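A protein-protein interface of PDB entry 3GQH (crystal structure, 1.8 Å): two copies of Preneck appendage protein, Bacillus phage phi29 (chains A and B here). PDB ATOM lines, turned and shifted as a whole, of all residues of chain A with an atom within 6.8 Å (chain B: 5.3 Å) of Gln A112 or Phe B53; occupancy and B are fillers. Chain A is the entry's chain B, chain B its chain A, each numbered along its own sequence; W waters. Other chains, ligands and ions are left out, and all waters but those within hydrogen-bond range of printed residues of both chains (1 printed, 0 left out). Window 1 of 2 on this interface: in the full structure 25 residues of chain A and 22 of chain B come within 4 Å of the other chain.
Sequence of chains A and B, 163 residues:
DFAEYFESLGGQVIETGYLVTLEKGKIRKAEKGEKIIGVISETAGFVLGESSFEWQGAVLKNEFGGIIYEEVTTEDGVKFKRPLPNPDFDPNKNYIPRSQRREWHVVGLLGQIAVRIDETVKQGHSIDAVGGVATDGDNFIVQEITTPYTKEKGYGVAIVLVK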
ATOM      1  N   ASP A   1      24.314  19.376   7.013  1.00  0.00           N
ATOM      2  CA  ASP A   1      23.971  18.650   8.275  1.00  0.00           C
ATOM      3  C   ASP A   1      22.612  19.066   8.803  1.00  0.00           C
ATOM      4  O   ASP A   1      22.113  20.147   8.484  1.00  0.00           O
ATOM      5  CB  ASP A   1      25.051  18.864   9.345  1.00  0.00           C
ATOM      6  CG  ASP A   1      25.478  20.326   9.475  1.00  0.00           C
ATOM      7  OD1 ASP A   1      25.484  20.844  10.606  1.00  0.00           O
ATOM      8  OD2 ASP A   1      25.830  20.946   8.449  1.00  0.00           O
ATOM      9  N   PHE A   2      22.021  18.191   9.609  1.00  0.00           N
ATOM     10  CA  PHE A   2      20.706  18.402  10.170  1.00  0.00           C
ATOM     11  C   PHE A   2      20.878  18.875  11.602  1.00  0.00           C
ATOM     12  O   PHE A   2      21.594  18.233  12.374  1.00  0.00           O
ATOM     13  CB  PHE A   2      19.921  17.096  10.106  1.00  0.00           C
ATOM     14  CG  PHE A   2      19.717  16.596   8.685  1.00  0.00           C
ATOM     15  CD1 PHE A   2      20.668  15.773   8.069  1.00  0.00           C
ATOM     16  CD2 PHE A   2      18.593  16.969   7.960  1.00  0.00           C
ATOM     17  CE1 PHE A   2      20.496  15.324   6.766  1.00  0.00           C
ATOM     18  CE2 PHE A   2      18.413  16.526   6.650  1.00  0.00           C
ATOM     19  CZ  PHE A   2      19.368  15.702   6.060  1.00  0.00           C
ATOM     20  N   SER A  41      27.460  24.243  14.676  1.00  0.00           N
ATOM     21  CA  SER A  41      27.568  24.221  13.215  1.00  0.00           C
ATOM     22  C   SER A  41      27.174  25.534  12.566  1.00  0.00           C
ATOM     23  O   SER A  41      26.233  26.183  13.012  1.00  0.00           O
ATOM     24  CB  SER A  41      26.663  23.122  12.660  1.00  0.00           C
ATOM     25  OG  SER A  41      26.781  23.046  11.250  1.00  0.00           O
ATOM     26  N   THR A  43      27.020  25.303   9.016  1.00  0.00           N
ATOM     27  CA  THR A  43      26.703  24.748   7.690  1.00  0.00           C
ATOM     28  C   THR A  43      25.338  24.055   7.613  1.00  0.00           C
ATOM     29  O   THR A  43      24.979  23.502   6.571  1.00  0.00           O
ATOM     30  CB  THR A  43      27.754  23.704   7.258  1.00  0.00           C
ATOM     31  OG1 THR A  43      27.866  22.686   8.271  1.00  0.00           O
ATOM     32  CG2 THR A  43      29.093  24.346   7.017  1.00  0.00           C
ATOM     33  N   LEU A 110      23.321  15.346  12.912  1.00  0.00           N
ATOM     34  CA  LEU A 110      23.467  14.266  11.946  1.00  0.00           C
ATOM     35  C   LEU A 110      24.067  14.835  10.680  1.00  0.00           C
ATOM     36  O   LEU A 110      23.595  15.858  10.185  1.00  0.00           O
ATOM     37  CB  LEU A 110      22.086  13.640  11.634  1.00  0.00           C
ATOM     38  CG  LEU A 110      22.006  12.657  10.427  1.00  0.00           C
ATOM     39  CD1 LEU A 110      22.829  11.436  10.676  1.00  0.00           C
ATOM     40  CD2 LEU A 110      20.556  12.278  10.114  1.00  0.00           C
ATOM     41  N   GLY A 111      25.091  14.163  10.156  1.00  0.00           N
ATOM     42  CA  GLY A 111      25.620  14.497   8.824  1.00  0.00           C
ATOM     43  C   GLY A 111      27.099  14.810   8.878  1.00  0.00           C
ATOM     44  O   GLY A 111      27.753  14.580   9.886  1.00  0.00           O
ATOM     45  N   GLN A 112      27.636  15.301   7.760  1.00  0.00           N
ATOM     46  CA  GLN A 112      29.054  15.617   7.683  1.00  0.00           C
ATOM     47  C   GLN A 112      29.250  17.004   8.277  1.00  0.00           C
ATOM     48  O   GLN A 112      28.677  17.985   7.788  1.00  0.00           O
ATOM     49  CB  GLN A 112      29.515  15.594   6.227  1.00  0.00           C
ATOM     50  CG  GLN A 112      29.213  14.264   5.542  1.00  0.00           C
ATOM     51  CD  GLN A 112      29.314  14.326   4.027  1.00  0.00           C
ATOM     52  OE1 GLN A 112      30.411  14.360   3.472  1.00  0.00           O
ATOM     53  NE2 GLN A 112      28.167  14.295   3.353  1.00  0.00           N
ATOM     54  N   ILE A 113      30.058  17.085   9.325  1.00  0.00           N
ATOM     55  CA  ILE A 113      30.192  18.340  10.075  1.00  0.00           C
ATOM     56  C   ILE A 113      31.675  18.625  10.356  1.00  0.00           C
ATOM     57  O   ILE A 113      32.438  17.713  10.627  1.00  0.00           O
ATOM     58  CB  ILE A 113      29.414  18.263  11.430  1.00  0.00           C
ATOM     59  CG1 ILE A 113      27.940  17.911  11.200  1.00  0.00           C
ATOM     60  CG2 ILE A 113      29.496  19.606  12.167  1.00  0.00           C
ATOM     61  CD1 ILE A 113      27.169  17.399  12.484  1.00  0.00           C
ATOM     62  N   ALA A 114      32.065  19.896  10.273  1.00  0.00           N
ATOM     63  CA  ALA A 114      33.435  20.304  10.580  1.00  0.00           C
ATOM     64  C   ALA A 114      33.641  20.377  12.099  1.00  0.00           C
ATOM     65  O   ALA A 114      32.834  20.979  12.820  1.00  0.00           O
ATOM     66  CB  ALA A 114      33.741  21.657   9.933  1.00  0.00           C
ATOM     67  N   GLN A 143      36.265  11.777   8.340  1.00  0.00           N
ATOM     68  CA  GLN A 143      36.253  11.683   6.877  1.00  0.00           C
ATOM     69  C   GLN A 143      37.540  12.196   6.270  1.00  0.00           C
ATOM     70  O   GLN A 143      38.174  11.514   5.469  1.00  0.00           O
ATOM     71  CB  GLN A 143      35.087  12.466   6.283  1.00  0.00           C
ATOM     72  CG  GLN A 143      33.803  11.728   6.325  1.00  0.00           C
ATOM     73  CD  GLN A 143      32.691  12.438   5.584  1.00  0.00           C
ATOM     74  OE1 GLN A 143      32.881  13.029   4.511  1.00  0.00           O
ATOM     75  NE2 GLN A 143      31.525  12.375   6.147  1.00  0.00           N
ATOM     76  N   THR A 146      40.806  18.685   6.915  1.00  0.00           N
ATOM     77  CA  THR A 146      40.769  19.744   5.916  1.00  0.00           C
ATOM     78  C   THR A 146      41.716  20.877   6.293  1.00  0.00           C
ATOM     79  O   THR A 146      42.251  21.569   5.414  1.00  0.00           O
ATOM     80  CB  THR A 146      39.332  20.267   5.699  1.00  0.00           C
ATOM     81  OG1 THR A 146      38.744  20.616   6.958  1.00  0.00           O
ATOM     82  CG2 THR A 146      38.459  19.204   5.023  1.00  0.00           C
ATOM     83  N   ILE A 159      36.439  17.009   8.791  1.00  0.00           N
ATOM     84  CA  ILE A 159      35.045  16.697   8.530  1.00  0.00           C
ATOM     85  C   ILE A 159      34.803  15.343   9.152  1.00  0.00           C
ATOM     86  O   ILE A 159      35.548  14.402   8.881  1.00  0.00           O
ATOM     87  CB  ILE A 159      34.733  16.612   7.024  1.00  0.00           C
ATOM     88  CG1 ILE A 159      35.096  17.929   6.304  1.00  0.00           C
ATOM     89  CG2 ILE A 159      33.277  16.220   6.815  1.00  0.00           C
ATOM     90  CD1 ILE A 159      34.515  19.182   6.946  1.00  0.00           C
ATOM     91  N   VAL A 160      33.780  15.270  10.004  1.00  0.00           N
ATOM     92  CA  VAL A 160      33.436  14.059  10.756  1.00  0.00           C
ATOM     93  C   VAL A 160      31.995  13.693  10.385  1.00  0.00           C
ATOM     94  O   VAL A 160      31.134  14.568  10.272  1.00  0.00           O
ATOM     95  CB  VAL A 160      33.587  14.303  12.277  1.00  0.00           C
ATOM     96  CG1 VAL A 160      33.083  13.127  13.114  1.00  0.00           C
ATOM     97  CG2 VAL A 160      35.065  14.576  12.630  1.00  0.00           C
ATOM     98  N   LEU A 161      31.730  12.407  10.166  1.00  0.00           N
ATOM     99  CA  LEU A 161      30.354  11.975   9.921  1.00  0.00           C
ATOM    100  C   LEU A 161      29.791  11.680  11.299  1.00  0.00           C
ATOM    101  O   LEU A 161      30.218  10.730  11.950  1.00  0.00           O
ATOM    102  CB  LEU A 161      30.281  10.728   9.019  1.00  0.00           C
ATOM    103  CG  LEU A 161      28.835  10.244   8.797  1.00  0.00           C
ATOM    104  CD1 LEU A 161      27.992  11.315   8.143  1.00  0.00           C
ATOM    105  CD2 LEU A 161      28.773   8.960   7.974  1.00  0.00           C
ATOM    106  N   VAL A 162      28.893  12.559  11.740  1.00  0.00           N
ATOM    107  CA  VAL A 162      28.198  12.460  13.027  1.00  0.00           C
ATOM    108  C   VAL A 162      26.842  11.779  12.849  1.00  0.00           C
ATOM    109  O   VAL A 162      26.068  12.131  11.959  1.00  0.00           O
ATOM    110  CB  VAL A 162      27.996  13.860  13.637  1.00  0.00           C
ATOM    111  CG1 VAL A 162      27.188  13.781  14.939  1.00  0.00           C
ATOM    112  CG2 VAL A 162      29.328  14.526  13.892  1.00  0.00           C
ATOM    113  N   GLU B   4      22.548  12.837   2.523  1.00  0.00           N
ATOM    114  CA  GLU B   4      23.572  13.809   2.105  1.00  0.00           C
ATOM    115  C   GLU B   4      24.327  13.289   0.895  1.00  0.00           C
ATOM    116  O   GLU B   4      24.302  12.102   0.595  1.00  0.00           O
ATOM    117  CB  GLU B   4      24.552  14.087   3.231  1.00  0.00           C
ATOM    118  CG  GLU B   4      23.882  14.804   4.423  1.00  0.00           C
ATOM    119  CD  GLU B   4      24.873  15.353   5.425  1.00  0.00           C
ATOM    120  OE1 GLU B   4      26.061  14.959   5.411  1.00  0.00           O
ATOM    121  OE2 GLU B   4      24.441  16.176   6.243  1.00  0.00           O
ATOM    122  N   TYR B   5      25.013  14.199   0.210  1.00  0.00           N
ATOM    123  CA  TYR B   5      25.879  13.792  -0.893  1.00  0.00           C
ATOM    124  C   TYR B   5      27.248  13.352  -0.393  1.00  0.00           C
ATOM    125  O   TYR B   5      27.881  14.050   0.411  1.00  0.00           O
ATOM    126  CB  TYR B   5      26.087  14.974  -1.833  1.00  0.00           C
ATOM    127  CG  TYR B   5      25.021  15.105  -2.870  1.00  0.00           C
ATOM    128  CD1 TYR B   5      24.022  16.075  -2.764  1.00  0.00           C
ATOM    129  CD2 TYR B   5      24.999  14.243  -3.959  1.00  0.00           C
ATOM    130  CE1 TYR B   5      23.025  16.192  -3.755  1.00  0.00           C
ATOM    131  CE2 TYR B   5      24.014  14.342  -4.934  1.00  0.00           C
ATOM    132  CZ  TYR B   5      23.041  15.311  -4.826  1.00  0.00           C
ATOM    133  OH  TYR B   5      22.085  15.385  -5.813  1.00  0.00           O
ATOM    134  N   PHE B   6      27.717  12.222  -0.923  1.00  0.00           N
ATOM    135  CA  PHE B   6      29.071  11.708  -0.694  1.00  0.00           C
ATOM    136  C   PHE B   6      29.659  11.276  -2.032  1.00  0.00           C
ATOM    137  O   PHE B   6      28.928  10.873  -2.919  1.00  0.00           O
ATOM    138  CB  PHE B   6      29.042  10.461   0.165  1.00  0.00           C
ATOM    139  CG  PHE B   6      28.579  10.689   1.586  1.00  0.00           C
ATOM    140  CD1 PHE B   6      27.215  10.743   1.888  1.00  0.00           C
ATOM    141  CD2 PHE B   6      29.512  10.796   2.601  1.00  0.00           C
ATOM    142  CE1 PHE B   6      26.780  10.914   3.208  1.00  0.00           C
ATOM    143  CE2 PHE B   6      29.105  10.967   3.917  1.00  0.00           C
ATOM    144  CZ  PHE B   6      27.732  11.037   4.217  1.00  0.00           C
ATOM    145  N   SER B  51      26.689  21.775  -1.978  1.00  0.00           N
ATOM    146  CA  SER B  51      27.780  22.735  -2.154  1.00  0.00           C
ATOM    147  C   SER B  51      28.566  22.967  -0.856  1.00  0.00           C
ATOM    148  O   SER B  51      29.279  23.966  -0.709  1.00  0.00           O
ATOM    149  CB  SER B  51      27.251  24.059  -2.724  1.00  0.00           C
ATOM    150  OG  SER B  51      26.373  24.706  -1.816  1.00  0.00           O
ATOM    151  N   SER B  52      28.436  22.026   0.077  1.00  0.00           N
ATOM    152  CA  SER B  52      29.141  22.095   1.354  1.00  0.00           C
ATOM    153  C   SER B  52      30.628  21.815   1.179  1.00  0.00           C
ATOM    154  O   SER B  52      31.021  21.016   0.325  1.00  0.00           O
ATOM    155  CB  SER B  52      28.551  21.085   2.334  1.00  0.00           C
ATOM    156  OG  SER B  52      28.800  19.765   1.882  1.00  0.00           O
ATOM    157  N   PHE B  53      31.438  22.480   2.000  1.00  0.00           N
ATOM    158  CA  PHE B  53      32.894  22.295   2.040  1.00  0.00           C
ATOM    159  C   PHE B  53      33.547  22.465   0.665  1.00  0.00           C
ATOM    160  O   PHE B  53      34.390  21.667   0.244  1.00  0.00           O
ATOM    161  CB  PHE B  53      33.267  20.971   2.733  1.00  0.00           C
ATOM    162  CG  PHE B  53      32.483  20.713   3.998  1.00  0.00           C
ATOM    163  CD1 PHE B  53      31.622  19.621   4.090  1.00  0.00           C
ATOM    164  CD2 PHE B  53      32.575  21.586   5.083  1.00  0.00           C
ATOM    165  CE1 PHE B  53      30.879  19.383   5.254  1.00  0.00           C
ATOM    166  CE2 PHE B  53      31.831  21.361   6.253  1.00  0.00           C
ATOM    167  CZ  PHE B  53      30.985  20.252   6.337  1.00  0.00           C
ATOM    168  N   GLU B  54      33.120  23.522  -0.023  1.00  0.00           N
ATOM    169  CA  GLU B  54      33.730  23.976  -1.265  1.00  0.00           C
ATOM    170  C   GLU B  54      34.522  25.260  -0.989  1.00  0.00           C
ATOM    171  O   GLU B  54      33.938  26.332  -0.809  1.00  0.00           O
ATOM    172  CB  GLU B  54      32.646  24.211  -2.331  1.00  0.00           C
ATOM    173  CG  GLU B  54      33.168  24.684  -3.693  1.00  0.00           C
ATOM    174  CD  GLU B  54      34.172  23.721  -4.314  1.00  0.00           C
ATOM    175  OE1 GLU B  54      33.810  22.549  -4.561  1.00  0.00           O
ATOM    176  OE2 GLU B  54      35.326  24.144  -4.554  1.00  0.00           O
ATOM    177  N   TRP B  55      35.845  25.145  -0.937  1.00  0.00           N
ATOM    178  CA  TRP B  55      36.698  26.309  -0.684  1.00  0.00           C
ATOM    179  C   TRP B  55      37.291  26.909  -1.969  1.00  0.00           C
ATOM    180  O   TRP B  55      38.316  27.598  -1.927  1.00  0.00           O
ATOM    181  CB  TRP B  55      37.795  25.977   0.338  1.00  0.00           C
ATOM    182  CG  TRP B  55      37.270  25.780   1.740  1.00  0.00           C
ATOM    183  CD1 TRP B  55      36.931  26.757   2.634  1.00  0.00           C
ATOM    184  CD2 TRP B  55      37.028  24.528   2.406  1.00  0.00           C
ATOM    185  NE1 TRP B  55      36.492  26.195   3.814  1.00  0.00           N
ATOM    186  CE2 TRP B  55      36.540  24.830   3.700  1.00  0.00           C
ATOM    187  CE3 TRP B  55      37.177  23.183   2.036  1.00  0.00           C
ATOM    188  CZ2 TRP B  55      36.198  23.834   4.626  1.00  0.00           C
ATOM    189  CZ3 TRP B  55      36.835  22.192   2.958  1.00  0.00           C
ATOM    190  CH2 TRP B  55      36.351  22.526   4.237  1.00  0.00           C
ATOM    191  N   PHE B  64      35.554  26.183   8.960  1.00  0.00           N
ATOM    192  CA  PHE B  64      34.420  25.310   9.347  1.00  0.00           C
ATOM    193  C   PHE B  64      33.320  25.205   8.285  1.00  0.00           C
ATOM    194  O   PHE B  64      32.265  24.591   8.519  1.00  0.00           O
ATOM    195  CB  PHE B  64      33.839  25.781  10.684  1.00  0.00           C
ATOM    196  CG  PHE B  64      34.832  25.769  11.786  1.00  0.00           C
ATOM    197  CD1 PHE B  64      35.241  24.565  12.357  1.00  0.00           C
ATOM    198  CD2 PHE B  64      35.400  26.952  12.232  1.00  0.00           C
ATOM    199  CE1 PHE B  64      36.177  24.538  13.377  1.00  0.00           C
ATOM    200  CE2 PHE B  64      36.338  26.942  13.257  1.00  0.00           C
ATOM    201  CZ  PHE B  64      36.736  25.731  13.832  1.00  0.00           C
ATOM    202  N   GLY B  65      33.578  25.791   7.115  1.00  0.00           N
ATOM    203  CA  GLY B  65      32.627  25.802   6.014  1.00  0.00           C
ATOM    204  C   GLY B  65      31.560  26.878   6.019  1.00  0.00           C
ATOM    205  O   GLY B  65      30.683  26.877   5.160  1.00  0.00           O
ATOM    206  N   ARG B  98      27.647  19.032  -8.181  1.00  0.00           N
ATOM    207  CA  ARG B  98      27.676  17.662  -7.652  1.00  0.00           C
ATOM    208  C   ARG B  98      26.503  16.808  -8.123  1.00  0.00           C
ATOM    209  O   ARG B  98      26.674  15.634  -8.464  1.00  0.00           O
ATOM    210  CB  ARG B  98      27.746  17.678  -6.117  1.00  0.00           C
ATOM    211  CG  ARG B  98      29.138  17.983  -5.609  1.00  0.00           C
ATOM    212  CD  ARG B  98      29.206  18.115  -4.098  1.00  0.00           C
ATOM    213  NE  ARG B  98      30.434  18.806  -3.704  1.00  0.00           N
ATOM    214  CZ  ARG B  98      30.666  19.326  -2.502  1.00  0.00           C
ATOM    215  NH1 ARG B  98      29.759  19.238  -1.533  1.00  0.00           N
ATOM    216  NH2 ARG B  98      31.817  19.940  -2.271  1.00  0.00           N
HETATM  217  O   HOH W   1      26.683  18.140   6.037  1.00  0.00           O
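O of Tyr B5 is in hydrogen-bond range of NE2 of Gln A112, at 3.0 Å.
The backbone NH of Gln A112 is in hydrogen-bond range of the side-chain carboxylate of Glu B4, at 2.8 Å.
The side-chain carboxylate (OE2) of Glu B4 sits close to the backbone NH (N) of Asp A1, at 3.3 Å.
The side-chain carboxylate (OD1) of Asp A1 sits at hydrogen-bond distance from the side-chain hydroxyl (OG) of Ser A41, at 2.6 Å.
O of Ile A159 is in hydrogen-bond range of N of Gln A143 (2.8 Å).
The backbone NH (N) of Gly A111 lies within hydrogen-bond range of the backbone carbonyl oxygen (O) of Val A162 (2.9 Å).
OG1 of Thr A43 sits at hydrogen-bond distance from OD2 of Asp A1, at 2.7 Å.
The side-chain amide oxygen (OE1) of Gln A112 lies close to the side-chain amide oxygen (OE1) of Gln A143, 3.0 Å away.
The side-chain hydroxyl (OG) of Ser A41 sits at hydrogen-bond distance from the backbone NH (N) of Thr A43 (3.2 Å).
Thr A43 touches Phe B64 (CG2 to O, 3.5 Å).
Thr A43 touches Gly B65.
Gly A111 touches Glu B4 (CA to OE2, 3.3 Å).
Phe B6 touches Gln A112 (CE2 to CD, 3.4 Å).
Gln A112 touches Phe B53.
Ala A114 touches Phe B64 (CB to O, 3.6 Å).
Gln A143 touches Phe B6.
CG2 of Thr A146 touches CZ3 of Trp B55 (3.98 Å).
Ile A159 touches Phe B53.
Leu A161 touches Phe B6 (CD1 to CZ, 3.9 Å).
Printed residues of chain B within 4 Å of Gly A111: Glu B4 (3.3 Å).
Of chain B, only Glu B4, Tyr B5, Phe B6 and Phe B53 come within 4 Å of Gln A112.
Printed residues of chain B within 4 Å of Thr A146: Trp B55 (3.98 Å).
Printed residues of chain A within 4 Å of Glu B4: Asp A1 (3.2 Å), Gly A111 (3.3 Å) and Gln A112 (2.8 Å).
Printed residues of chain A within 4 Å of Tyr B5: Gln A112.
Printed residues of chain A within 4 Å of Phe B6: Gln A112, Gln A143 and Leu A161.
The nearest printed residue of chain B that does not touch Gln A112 is Ser B52 (5.7 Å).
The nearest printed residue of chain A that does not touch Phe B53 is Ala A114 (4.1 Å).
The nearest printed residue of chain A that does not touch Trp B55 is Ile A159 (4.7 Å).
Of the 15 printed residues of chain A, 9 touch a printed residue of chain B.
Printed residues of chain A that touch a printed residue of chain B: Asp A1, Thr A43, Gly A111, Gln A112, Ala A114, Gln A143, Thr A146, Ile A159 and Leu A161.
Of the 11 printed residues of chain B, 7 touch a printed residue of chain A.
Hydrophobic or aromatic side chains of chain B that line the printed part of chain A: Phe B6, Phe B53 and Trp B55.
Among the printed residues, 13 pairs touch across the chains.
Among the printed residues, no Asp or Glu carboxylate lies within 4 Å of a Lys or Arg side-chain nitrogen of the other chain.
No position is printed for both chains.
Of the 13 pairs that touch across the chains among the printed residues, none has its exchanged pair printed and touching as well.
Water W1 lies within hydrogen-bond range of the backbone carbonyl oxygen (O) of Gln A112 (2.7 Å), the backbone NH (N) of Asp A1 (2.8 Å) and the side-chain carboxylate (OE2) of Glu B4 (3.0 Å).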
